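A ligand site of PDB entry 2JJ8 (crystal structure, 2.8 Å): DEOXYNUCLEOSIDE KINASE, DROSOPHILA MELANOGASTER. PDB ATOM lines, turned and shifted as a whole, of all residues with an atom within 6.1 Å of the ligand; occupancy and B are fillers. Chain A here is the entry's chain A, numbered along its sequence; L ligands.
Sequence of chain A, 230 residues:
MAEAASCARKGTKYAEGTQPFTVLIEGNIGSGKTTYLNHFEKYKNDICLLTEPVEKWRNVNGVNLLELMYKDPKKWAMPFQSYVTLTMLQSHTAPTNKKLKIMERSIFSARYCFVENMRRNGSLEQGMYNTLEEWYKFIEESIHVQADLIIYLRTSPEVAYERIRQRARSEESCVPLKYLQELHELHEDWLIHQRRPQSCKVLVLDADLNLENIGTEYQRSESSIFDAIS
The backbone NH (N) of Phe 114 is in hydrogen-bond range of the backbone carbonyl oxygen (O) of Ser 109 (3.2 Å).
O of Trp 57 lies within hydrogen-bond range of N of Leu 66 (3.5 Å).
OE2 of Glu 52 is in salt-bridge range of NH1 of Arg 105 (2.6 Å).
N of Val 115 lies within hydrogen-bond range of O of Ala 110 (2.9 Å).
The side-chain sulfur (SD) of Met 118 sits close to the side-chain amide oxygen (OE1) of Gln 81 (3.5 Å).
Merely in contact with the ligand: Phe 80 (3.1 Å), Phe 114 (3.3 Å), Ala 110 (3.3 Å), Trp 57 (3.5 Å), Val 84 (3.6 Å), Arg 105 (3.6 Å), Met 88 (3.8 Å) and Val 54 (3.9 Å).
Hydrophobic or aromatic side chains that line the ligand: Val 54, Trp 57, Phe 80, Val 84, Met 88, Ala 110 and Phe 114.
OE1 of Glu 52 is in hydrogen-bond range of O1 of the ligand (2.8 Å).
A nitrogen (N5) of the ligand sits at hydrogen-bond distance from the side-chain amide oxygen (OE1) of Gln 81 (2.9 Å).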
ATOM      1  N   ILE A  29      -0.516  17.914  15.143  1.00  0.00           N
ATOM      2  CA  ILE A  29      -0.646  19.278  15.669  1.00  0.00           C
ATOM      3  C   ILE A  29      -2.007  19.349  16.366  1.00  0.00           C
ATOM      4  O   ILE A  29      -3.034  18.960  15.791  1.00  0.00           O
ATOM      5  CB  ILE A  29      -0.539  20.353  14.562  1.00  0.00           C
ATOM      6  CG1 ILE A  29       0.764  20.168  13.756  1.00  0.00           C
ATOM      7  CG2 ILE A  29      -0.654  21.770  15.146  1.00  0.00           C
ATOM      8  CD1 ILE A  29       0.807  20.911  12.420  1.00  0.00           C
ATOM      9  N   LYS A  33      -0.389  17.643  23.097  1.00  0.00           N
ATOM     10  CA  LYS A  33       0.969  17.274  23.541  1.00  0.00           C
ATOM     11  C   LYS A  33       1.528  18.152  24.645  1.00  0.00           C
ATOM     12  O   LYS A  33       2.170  17.646  25.567  1.00  0.00           O
ATOM     13  CB  LYS A  33       1.956  17.279  22.370  1.00  0.00           C
ATOM     14  CG  LYS A  33       1.884  16.054  21.470  1.00  0.00           C
ATOM     15  CD  LYS A  33       2.928  16.128  20.366  1.00  0.00           C
ATOM     16  CE  LYS A  33       2.394  16.814  19.134  1.00  0.00           C
ATOM     17  NZ  LYS A  33       2.295  18.273  19.245  1.00  0.00           N
ATOM     18  N   GLU A  52       9.298  20.549  22.581  1.00  0.00           N
ATOM     19  CA  GLU A  52       9.707  20.796  21.196  1.00  0.00           C
ATOM     20  C   GLU A  52      10.412  22.159  21.110  1.00  0.00           C
ATOM     21  O   GLU A  52       9.883  23.146  21.579  1.00  0.00           O
ATOM     22  CB  GLU A  52       8.452  20.791  20.334  1.00  0.00           C
ATOM     23  CG  GLU A  52       8.660  20.389  18.887  1.00  0.00           C
ATOM     24  CD  GLU A  52       7.379  20.521  18.046  1.00  0.00           C
ATOM     25  OE1 GLU A  52       6.621  21.487  18.260  1.00  0.00           O
ATOM     26  OE2 GLU A  52       7.134  19.661  17.179  1.00  0.00           O
ATOM     27  N   VAL A  54      10.662  24.829  19.491  1.00  0.00           N
ATOM     28  CA  VAL A  54      10.094  25.882  18.650  1.00  0.00           C
ATOM     29  C   VAL A  54      10.788  27.218  18.908  1.00  0.00           C
ATOM     30  O   VAL A  54      11.010  27.973  17.983  1.00  0.00           O
ATOM     31  CB  VAL A  54       8.590  26.081  18.911  1.00  0.00           C
ATOM     32  CG1 VAL A  54       7.855  26.342  17.603  1.00  0.00           C
ATOM     33  CG2 VAL A  54       7.979  24.872  19.610  1.00  0.00           C
ATOM     34  N   TRP A  57      13.748  27.404  16.930  1.00  0.00           N
ATOM     35  CA  TRP A  57      13.396  27.635  15.518  1.00  0.00           C
ATOM     36  C   TRP A  57      12.967  29.092  15.238  1.00  0.00           C
ATOM     37  O   TRP A  57      13.183  29.602  14.138  1.00  0.00           O
ATOM     38  CB  TRP A  57      12.336  26.664  15.002  1.00  0.00           C
ATOM     39  CG  TRP A  57      12.523  25.246  15.416  1.00  0.00           C
ATOM     40  CD1 TRP A  57      13.677  24.641  15.760  1.00  0.00           C
ATOM     41  CD2 TRP A  57      11.512  24.241  15.502  1.00  0.00           C
ATOM     42  NE1 TRP A  57      13.461  23.322  16.071  1.00  0.00           N
ATOM     43  CE2 TRP A  57      12.127  23.059  15.927  1.00  0.00           C
ATOM     44  CE3 TRP A  57      10.137  24.243  15.265  1.00  0.00           C
ATOM     45  CZ2 TRP A  57      11.421  21.874  16.140  1.00  0.00           C
ATOM     46  CZ3 TRP A  57       9.427  23.065  15.473  1.00  0.00           C
ATOM     47  CH2 TRP A  57      10.070  21.904  15.904  1.00  0.00           C
ATOM     48  N   LEU A  66      10.957  29.771  11.484  1.00  0.00           N
ATOM     49  CA  LEU A  66       9.561  29.307  11.418  1.00  0.00           C
ATOM     50  C   LEU A  66       8.718  30.203  10.473  1.00  0.00           C
ATOM     51  O   LEU A  66       8.122  29.681   9.524  1.00  0.00           O
ATOM     52  CB  LEU A  66       8.952  29.220  12.823  1.00  0.00           C
ATOM     53  CG  LEU A  66       7.660  28.436  13.004  1.00  0.00           C
ATOM     54  CD1 LEU A  66       7.674  27.111  12.253  1.00  0.00           C
ATOM     55  CD2 LEU A  66       7.400  28.205  14.478  1.00  0.00           C
ATOM     56  N   MET A  69       9.473  30.042   6.819  1.00  0.00           N
ATOM     57  CA  MET A  69       9.090  28.791   6.204  1.00  0.00           C
ATOM     58  C   MET A  69       7.641  28.872   5.743  1.00  0.00           C
ATOM     59  O   MET A  69       7.280  28.451   4.612  1.00  0.00           O
ATOM     60  CB  MET A  69       9.304  27.644   7.182  1.00  0.00           C
ATOM     61  CG  MET A  69       9.629  26.337   6.540  1.00  0.00           C
ATOM     62  SD  MET A  69       8.145  25.505   5.993  1.00  0.00           S
ATOM     63  CE  MET A  69       7.168  25.400   7.502  1.00  0.00           C
ATOM     64  N   PHE A  80      14.999  25.080   7.230  1.00  0.00           N
ATOM     65  CA  PHE A  80      14.156  24.870   8.398  1.00  0.00           C
ATOM     66  C   PHE A  80      14.217  23.427   8.934  1.00  0.00           C
ATOM     67  O   PHE A  80      14.513  23.208  10.110  1.00  0.00           O
ATOM     68  CB  PHE A  80      12.719  25.303   8.103  1.00  0.00           C
ATOM     69  CG  PHE A  80      11.746  24.954   9.190  1.00  0.00           C
ATOM     70  CD1 PHE A  80      11.804  25.604  10.425  1.00  0.00           C
ATOM     71  CD2 PHE A  80      10.799  23.974   8.979  1.00  0.00           C
ATOM     72  CE1 PHE A  80      10.905  25.271  11.453  1.00  0.00           C
ATOM     73  CE2 PHE A  80       9.899  23.627   9.992  1.00  0.00           C
ATOM     74  CZ  PHE A  80       9.948  24.281  11.238  1.00  0.00           C
ATOM     75  N   GLN A  81      13.946  22.448   8.075  1.00  0.00           N
ATOM     76  CA  GLN A  81      13.931  21.030   8.483  1.00  0.00           C
ATOM     77  C   GLN A  81      15.320  20.562   8.862  1.00  0.00           C
ATOM     78  O   GLN A  81      15.471  19.800   9.794  1.00  0.00           O
ATOM     79  CB  GLN A  81      13.340  20.134   7.397  1.00  0.00           C
ATOM     80  CG  GLN A  81      11.850  20.325   7.136  1.00  0.00           C
ATOM     81  CD  GLN A  81      10.988  20.062   8.360  1.00  0.00           C
ATOM     82  OE1 GLN A  81       9.940  20.682   8.508  1.00  0.00           O
ATOM     83  NE2 GLN A  81      11.423  19.153   9.241  1.00  0.00           N
ATOM     84  N   VAL A  84      15.601  21.939  12.322  1.00  0.00           N
ATOM     85  CA  VAL A  84      14.765  21.132  13.222  1.00  0.00           C
ATOM     86  C   VAL A  84      15.528  19.860  13.576  1.00  0.00           C
ATOM     87  O   VAL A  84      15.674  19.533  14.764  1.00  0.00           O
ATOM     88  CB  VAL A  84      13.407  20.773  12.617  1.00  0.00           C
ATOM     89  CG1 VAL A  84      12.709  19.790  13.465  1.00  0.00           C
ATOM     90  CG2 VAL A  84      12.548  22.008  12.456  1.00  0.00           C
ATOM     91  N   MET A  88      16.597  18.614  17.354  1.00  0.00           N
ATOM     92  CA  MET A  88      16.166  17.341  17.880  1.00  0.00           C
ATOM     93  C   MET A  88      17.375  16.600  18.407  1.00  0.00           C
ATOM     94  O   MET A  88      17.345  16.097  19.535  1.00  0.00           O
ATOM     95  CB  MET A  88      15.442  16.526  16.806  1.00  0.00           C
ATOM     96  CG  MET A  88      14.071  17.084  16.405  1.00  0.00           C
ATOM     97  SD  MET A  88      13.002  17.371  17.827  1.00  0.00           S
ATOM     98  CE  MET A  88      11.467  17.835  17.041  1.00  0.00           C
ATOM     99  N   ARG A 105       7.934  15.368  20.770  1.00  0.00           N
ATOM    100  CA  ARG A 105       8.416  15.110  19.410  1.00  0.00           C
ATOM    101  C   ARG A 105       9.888  14.692  19.418  1.00  0.00           C
ATOM    102  O   ARG A 105      10.504  14.586  20.472  1.00  0.00           O
ATOM    103  CB  ARG A 105       8.143  16.285  18.480  1.00  0.00           C
ATOM    104  CG  ARG A 105       6.659  16.472  18.170  1.00  0.00           C
ATOM    105  CD  ARG A 105       6.422  16.599  16.675  1.00  0.00           C
ATOM    106  NE  ARG A 105       5.009  16.589  16.323  1.00  0.00           N
ATOM    107  CZ  ARG A 105       4.240  17.674  16.185  1.00  0.00           C
ATOM    108  NH1 ARG A 105       4.741  18.884  16.410  1.00  0.00           N
ATOM    109  NH2 ARG A 105       2.964  17.557  15.840  1.00  0.00           N
ATOM    110  N   SER A 106      10.433  14.441  18.240  1.00  0.00           N
ATOM    111  CA  SER A 106      11.731  13.788  18.107  1.00  0.00           C
ATOM    112  C   SER A 106      12.268  13.954  16.697  1.00  0.00           C
ATOM    113  O   SER A 106      11.592  14.517  15.823  1.00  0.00           O
ATOM    114  CB  SER A 106      11.567  12.300  18.316  1.00  0.00           C
ATOM    115  OG  SER A 106      10.838  11.777  17.214  1.00  0.00           O
ATOM    116  N   SER A 109       9.719  12.001  14.288  1.00  0.00           N
ATOM    117  CA  SER A 109       8.541  12.664  13.745  1.00  0.00           C
ATOM    118  C   SER A 109       8.966  13.641  12.659  1.00  0.00           C
ATOM    119  O   SER A 109       8.331  13.680  11.585  1.00  0.00           O
ATOM    120  CB  SER A 109       7.622  13.327  14.810  1.00  0.00           C
ATOM    121  OG  SER A 109       8.323  13.805  15.951  1.00  0.00           O
ATOM    122  N   ALA A 110      10.043  14.373  12.914  1.00  0.00           N
ATOM    123  CA  ALA A 110      10.578  15.318  11.921  1.00  0.00           C
ATOM    124  C   ALA A 110      10.888  14.662  10.589  1.00  0.00           C
ATOM    125  O   ALA A 110      10.534  15.206   9.544  1.00  0.00           O
ATOM    126  CB  ALA A 110      11.802  16.034  12.445  1.00  0.00           C
ATOM    127  N   ARG A 111      11.501  13.484  10.613  1.00  0.00           N
ATOM    128  CA  ARG A 111      11.817  12.765   9.396  1.00  0.00           C
ATOM    129  C   ARG A 111      10.596  12.132   8.740  1.00  0.00           C
ATOM    130  O   ARG A 111      10.265  12.430   7.569  1.00  0.00           O
ATOM    131  CB  ARG A 111      12.879  11.692   9.650  1.00  0.00           C
ATOM    132  CG  ARG A 111      13.178  10.834   8.444  1.00  0.00           C
ATOM    133  CD  ARG A 111      14.230   9.824   8.790  1.00  0.00           C
ATOM    134  NE  ARG A 111      14.707   9.144   7.590  1.00  0.00           N
ATOM    135  CZ  ARG A 111      15.558   8.128   7.587  1.00  0.00           C
ATOM    136  NH1 ARG A 111      16.050   7.641   8.728  1.00  0.00           N
ATOM    137  NH2 ARG A 111      15.921   7.593   6.450  1.00  0.00           N
ATOM    138  N   PHE A 114       7.007  15.185   9.117  1.00  0.00           N
ATOM    139  CA  PHE A 114       7.054  16.539   8.525  1.00  0.00           C
ATOM    140  C   PHE A 114       7.858  16.652   7.221  1.00  0.00           C
ATOM    141  O   PHE A 114       7.402  17.290   6.252  1.00  0.00           O
ATOM    142  CB  PHE A 114       7.486  17.579   9.577  1.00  0.00           C
ATOM    143  CG  PHE A 114       6.477  17.773  10.680  1.00  0.00           C
ATOM    144  CD1 PHE A 114       6.525  16.990  11.833  1.00  0.00           C
ATOM    145  CD2 PHE A 114       5.442  18.691  10.548  1.00  0.00           C
ATOM    146  CE1 PHE A 114       5.562  17.146  12.847  1.00  0.00           C
ATOM    147  CE2 PHE A 114       4.469  18.849  11.536  1.00  0.00           C
ATOM    148  CZ  PHE A 114       4.541  18.070  12.695  1.00  0.00           C
ATOM    149  N   VAL A 115       9.031  16.009   7.183  1.00  0.00           N
ATOM    150  CA  VAL A 115       9.867  16.044   5.989  1.00  0.00           C
ATOM    151  C   VAL A 115       9.188  15.255   4.877  1.00  0.00           C
ATOM    152  O   VAL A 115       9.072  15.727   3.750  1.00  0.00           O
ATOM    153  CB  VAL A 115      11.320  15.531   6.256  1.00  0.00           C
ATOM    154  CG1 VAL A 115      12.008  15.086   4.962  1.00  0.00           C
ATOM    155  CG2 VAL A 115      12.130  16.600   6.936  1.00  0.00           C
ATOM    156  N   MET A 118       6.399  17.134   3.337  1.00  0.00           N
ATOM    157  CA  MET A 118       6.892  18.228   2.485  1.00  0.00           C
ATOM    158  C   MET A 118       7.390  17.722   1.130  1.00  0.00           C
ATOM    159  O   MET A 118       7.328  18.451   0.138  1.00  0.00           O
ATOM    160  CB  MET A 118       7.970  19.045   3.187  1.00  0.00           C
ATOM    161  CG  MET A 118       7.432  20.108   4.098  1.00  0.00           C
ATOM    162  SD  MET A 118       8.718  20.701   5.204  1.00  0.00           S
ATOM    163  CE  MET A 118       7.771  21.826   6.209  1.00  0.00           C
ATOM    164  N   VAL A 175      -4.042  26.058  11.033  1.00  0.00           N
ATOM    165  CA  VAL A 175      -3.496  25.269   9.927  1.00  0.00           C
ATOM    166  C   VAL A 175      -4.685  24.651   9.192  1.00  0.00           C
ATOM    167  O   VAL A 175      -5.706  24.336   9.805  1.00  0.00           O
ATOM    168  CB  VAL A 175      -2.573  24.135  10.450  1.00  0.00           C
ATOM    169  CG1 VAL A 175      -1.455  23.867   9.459  1.00  0.00           C
ATOM    170  CG2 VAL A 175      -1.984  24.499  11.823  1.00  0.00           C
ATOM    171  N   TYR A 179      -3.913  19.481   5.639  1.00  0.00           N
ATOM    172  CA  TYR A 179      -2.576  19.332   6.191  1.00  0.00           C
ATOM    173  C   TYR A 179      -2.595  18.384   7.380  1.00  0.00           C
ATOM    174  O   TYR A 179      -1.788  17.460   7.462  1.00  0.00           O
ATOM    175  CB  TYR A 179      -2.026  20.705   6.576  1.00  0.00           C
ATOM    176  CG  TYR A 179      -0.574  20.723   6.982  1.00  0.00           C
ATOM    177  CD1 TYR A 179       0.445  20.360   6.091  1.00  0.00           C
ATOM    178  CD2 TYR A 179      -0.204  21.156   8.270  1.00  0.00           C
ATOM    179  CE1 TYR A 179       1.800  20.398   6.490  1.00  0.00           C
ATOM    180  CE2 TYR A 179       1.143  21.215   8.667  1.00  0.00           C
ATOM    181  CZ  TYR A 179       2.137  20.823   7.775  1.00  0.00           C
ATOM    182  OH  TYR A 179       3.466  20.876   8.178  1.00  0.00           O
HETATM  183  O1  LIG L   1       5.192  22.491  16.129  1.00  0.00           O
HETATM  184  C1  LIG L   1       5.405  23.885  15.848  1.00  0.00           C
HETATM  185  C2  LIG L   1       5.324  24.070  14.343  1.00  0.00           C
HETATM  186  O2  LIG L   1       6.454  23.517  13.683  1.00  0.00           O
HETATM  187  C3  LIG L   1       4.116  23.312  13.825  1.00  0.00           C
HETATM  188  N1  LIG L   1       3.295  24.342  13.247  1.00  0.00           N
HETATM  189  N2  LIG L   1       2.415  25.088  13.727  1.00  0.00           N
HETATM  190  N3  LIG L   1       1.651  25.743  14.139  1.00  0.00           N
HETATM  191  C4  LIG L   1       4.606  22.284  12.814  1.00  0.00           C
HETATM  192  C5  LIG L   1       6.085  22.632  12.604  1.00  0.00           C
HETATM  193  N4  LIG L   1       7.049  21.512  12.482  1.00  0.00           N
HETATM  194  C6  LIG L   1       7.648  21.269  11.214  1.00  0.00           C
HETATM  195  O3  LIG L   1       7.320  21.972  10.231  1.00  0.00           O
HETATM  196  N5  LIG L   1       8.555  20.303  11.011  1.00  0.00           N
HETATM  197  C7  LIG L   1       8.940  19.508  12.011  1.00  0.00           C
HETATM  198  O4  LIG L   1       9.793  18.609  11.811  1.00  0.00           O
HETATM  199  C8  LIG L   1       8.340  19.738  13.354  1.00  0.00           C
HETATM  200  C9  LIG L   1       8.762  18.853  14.499  1.00  0.00           C
HETATM  201  C10 LIG L   1       7.413  20.770  13.531  1.00  0.00           C
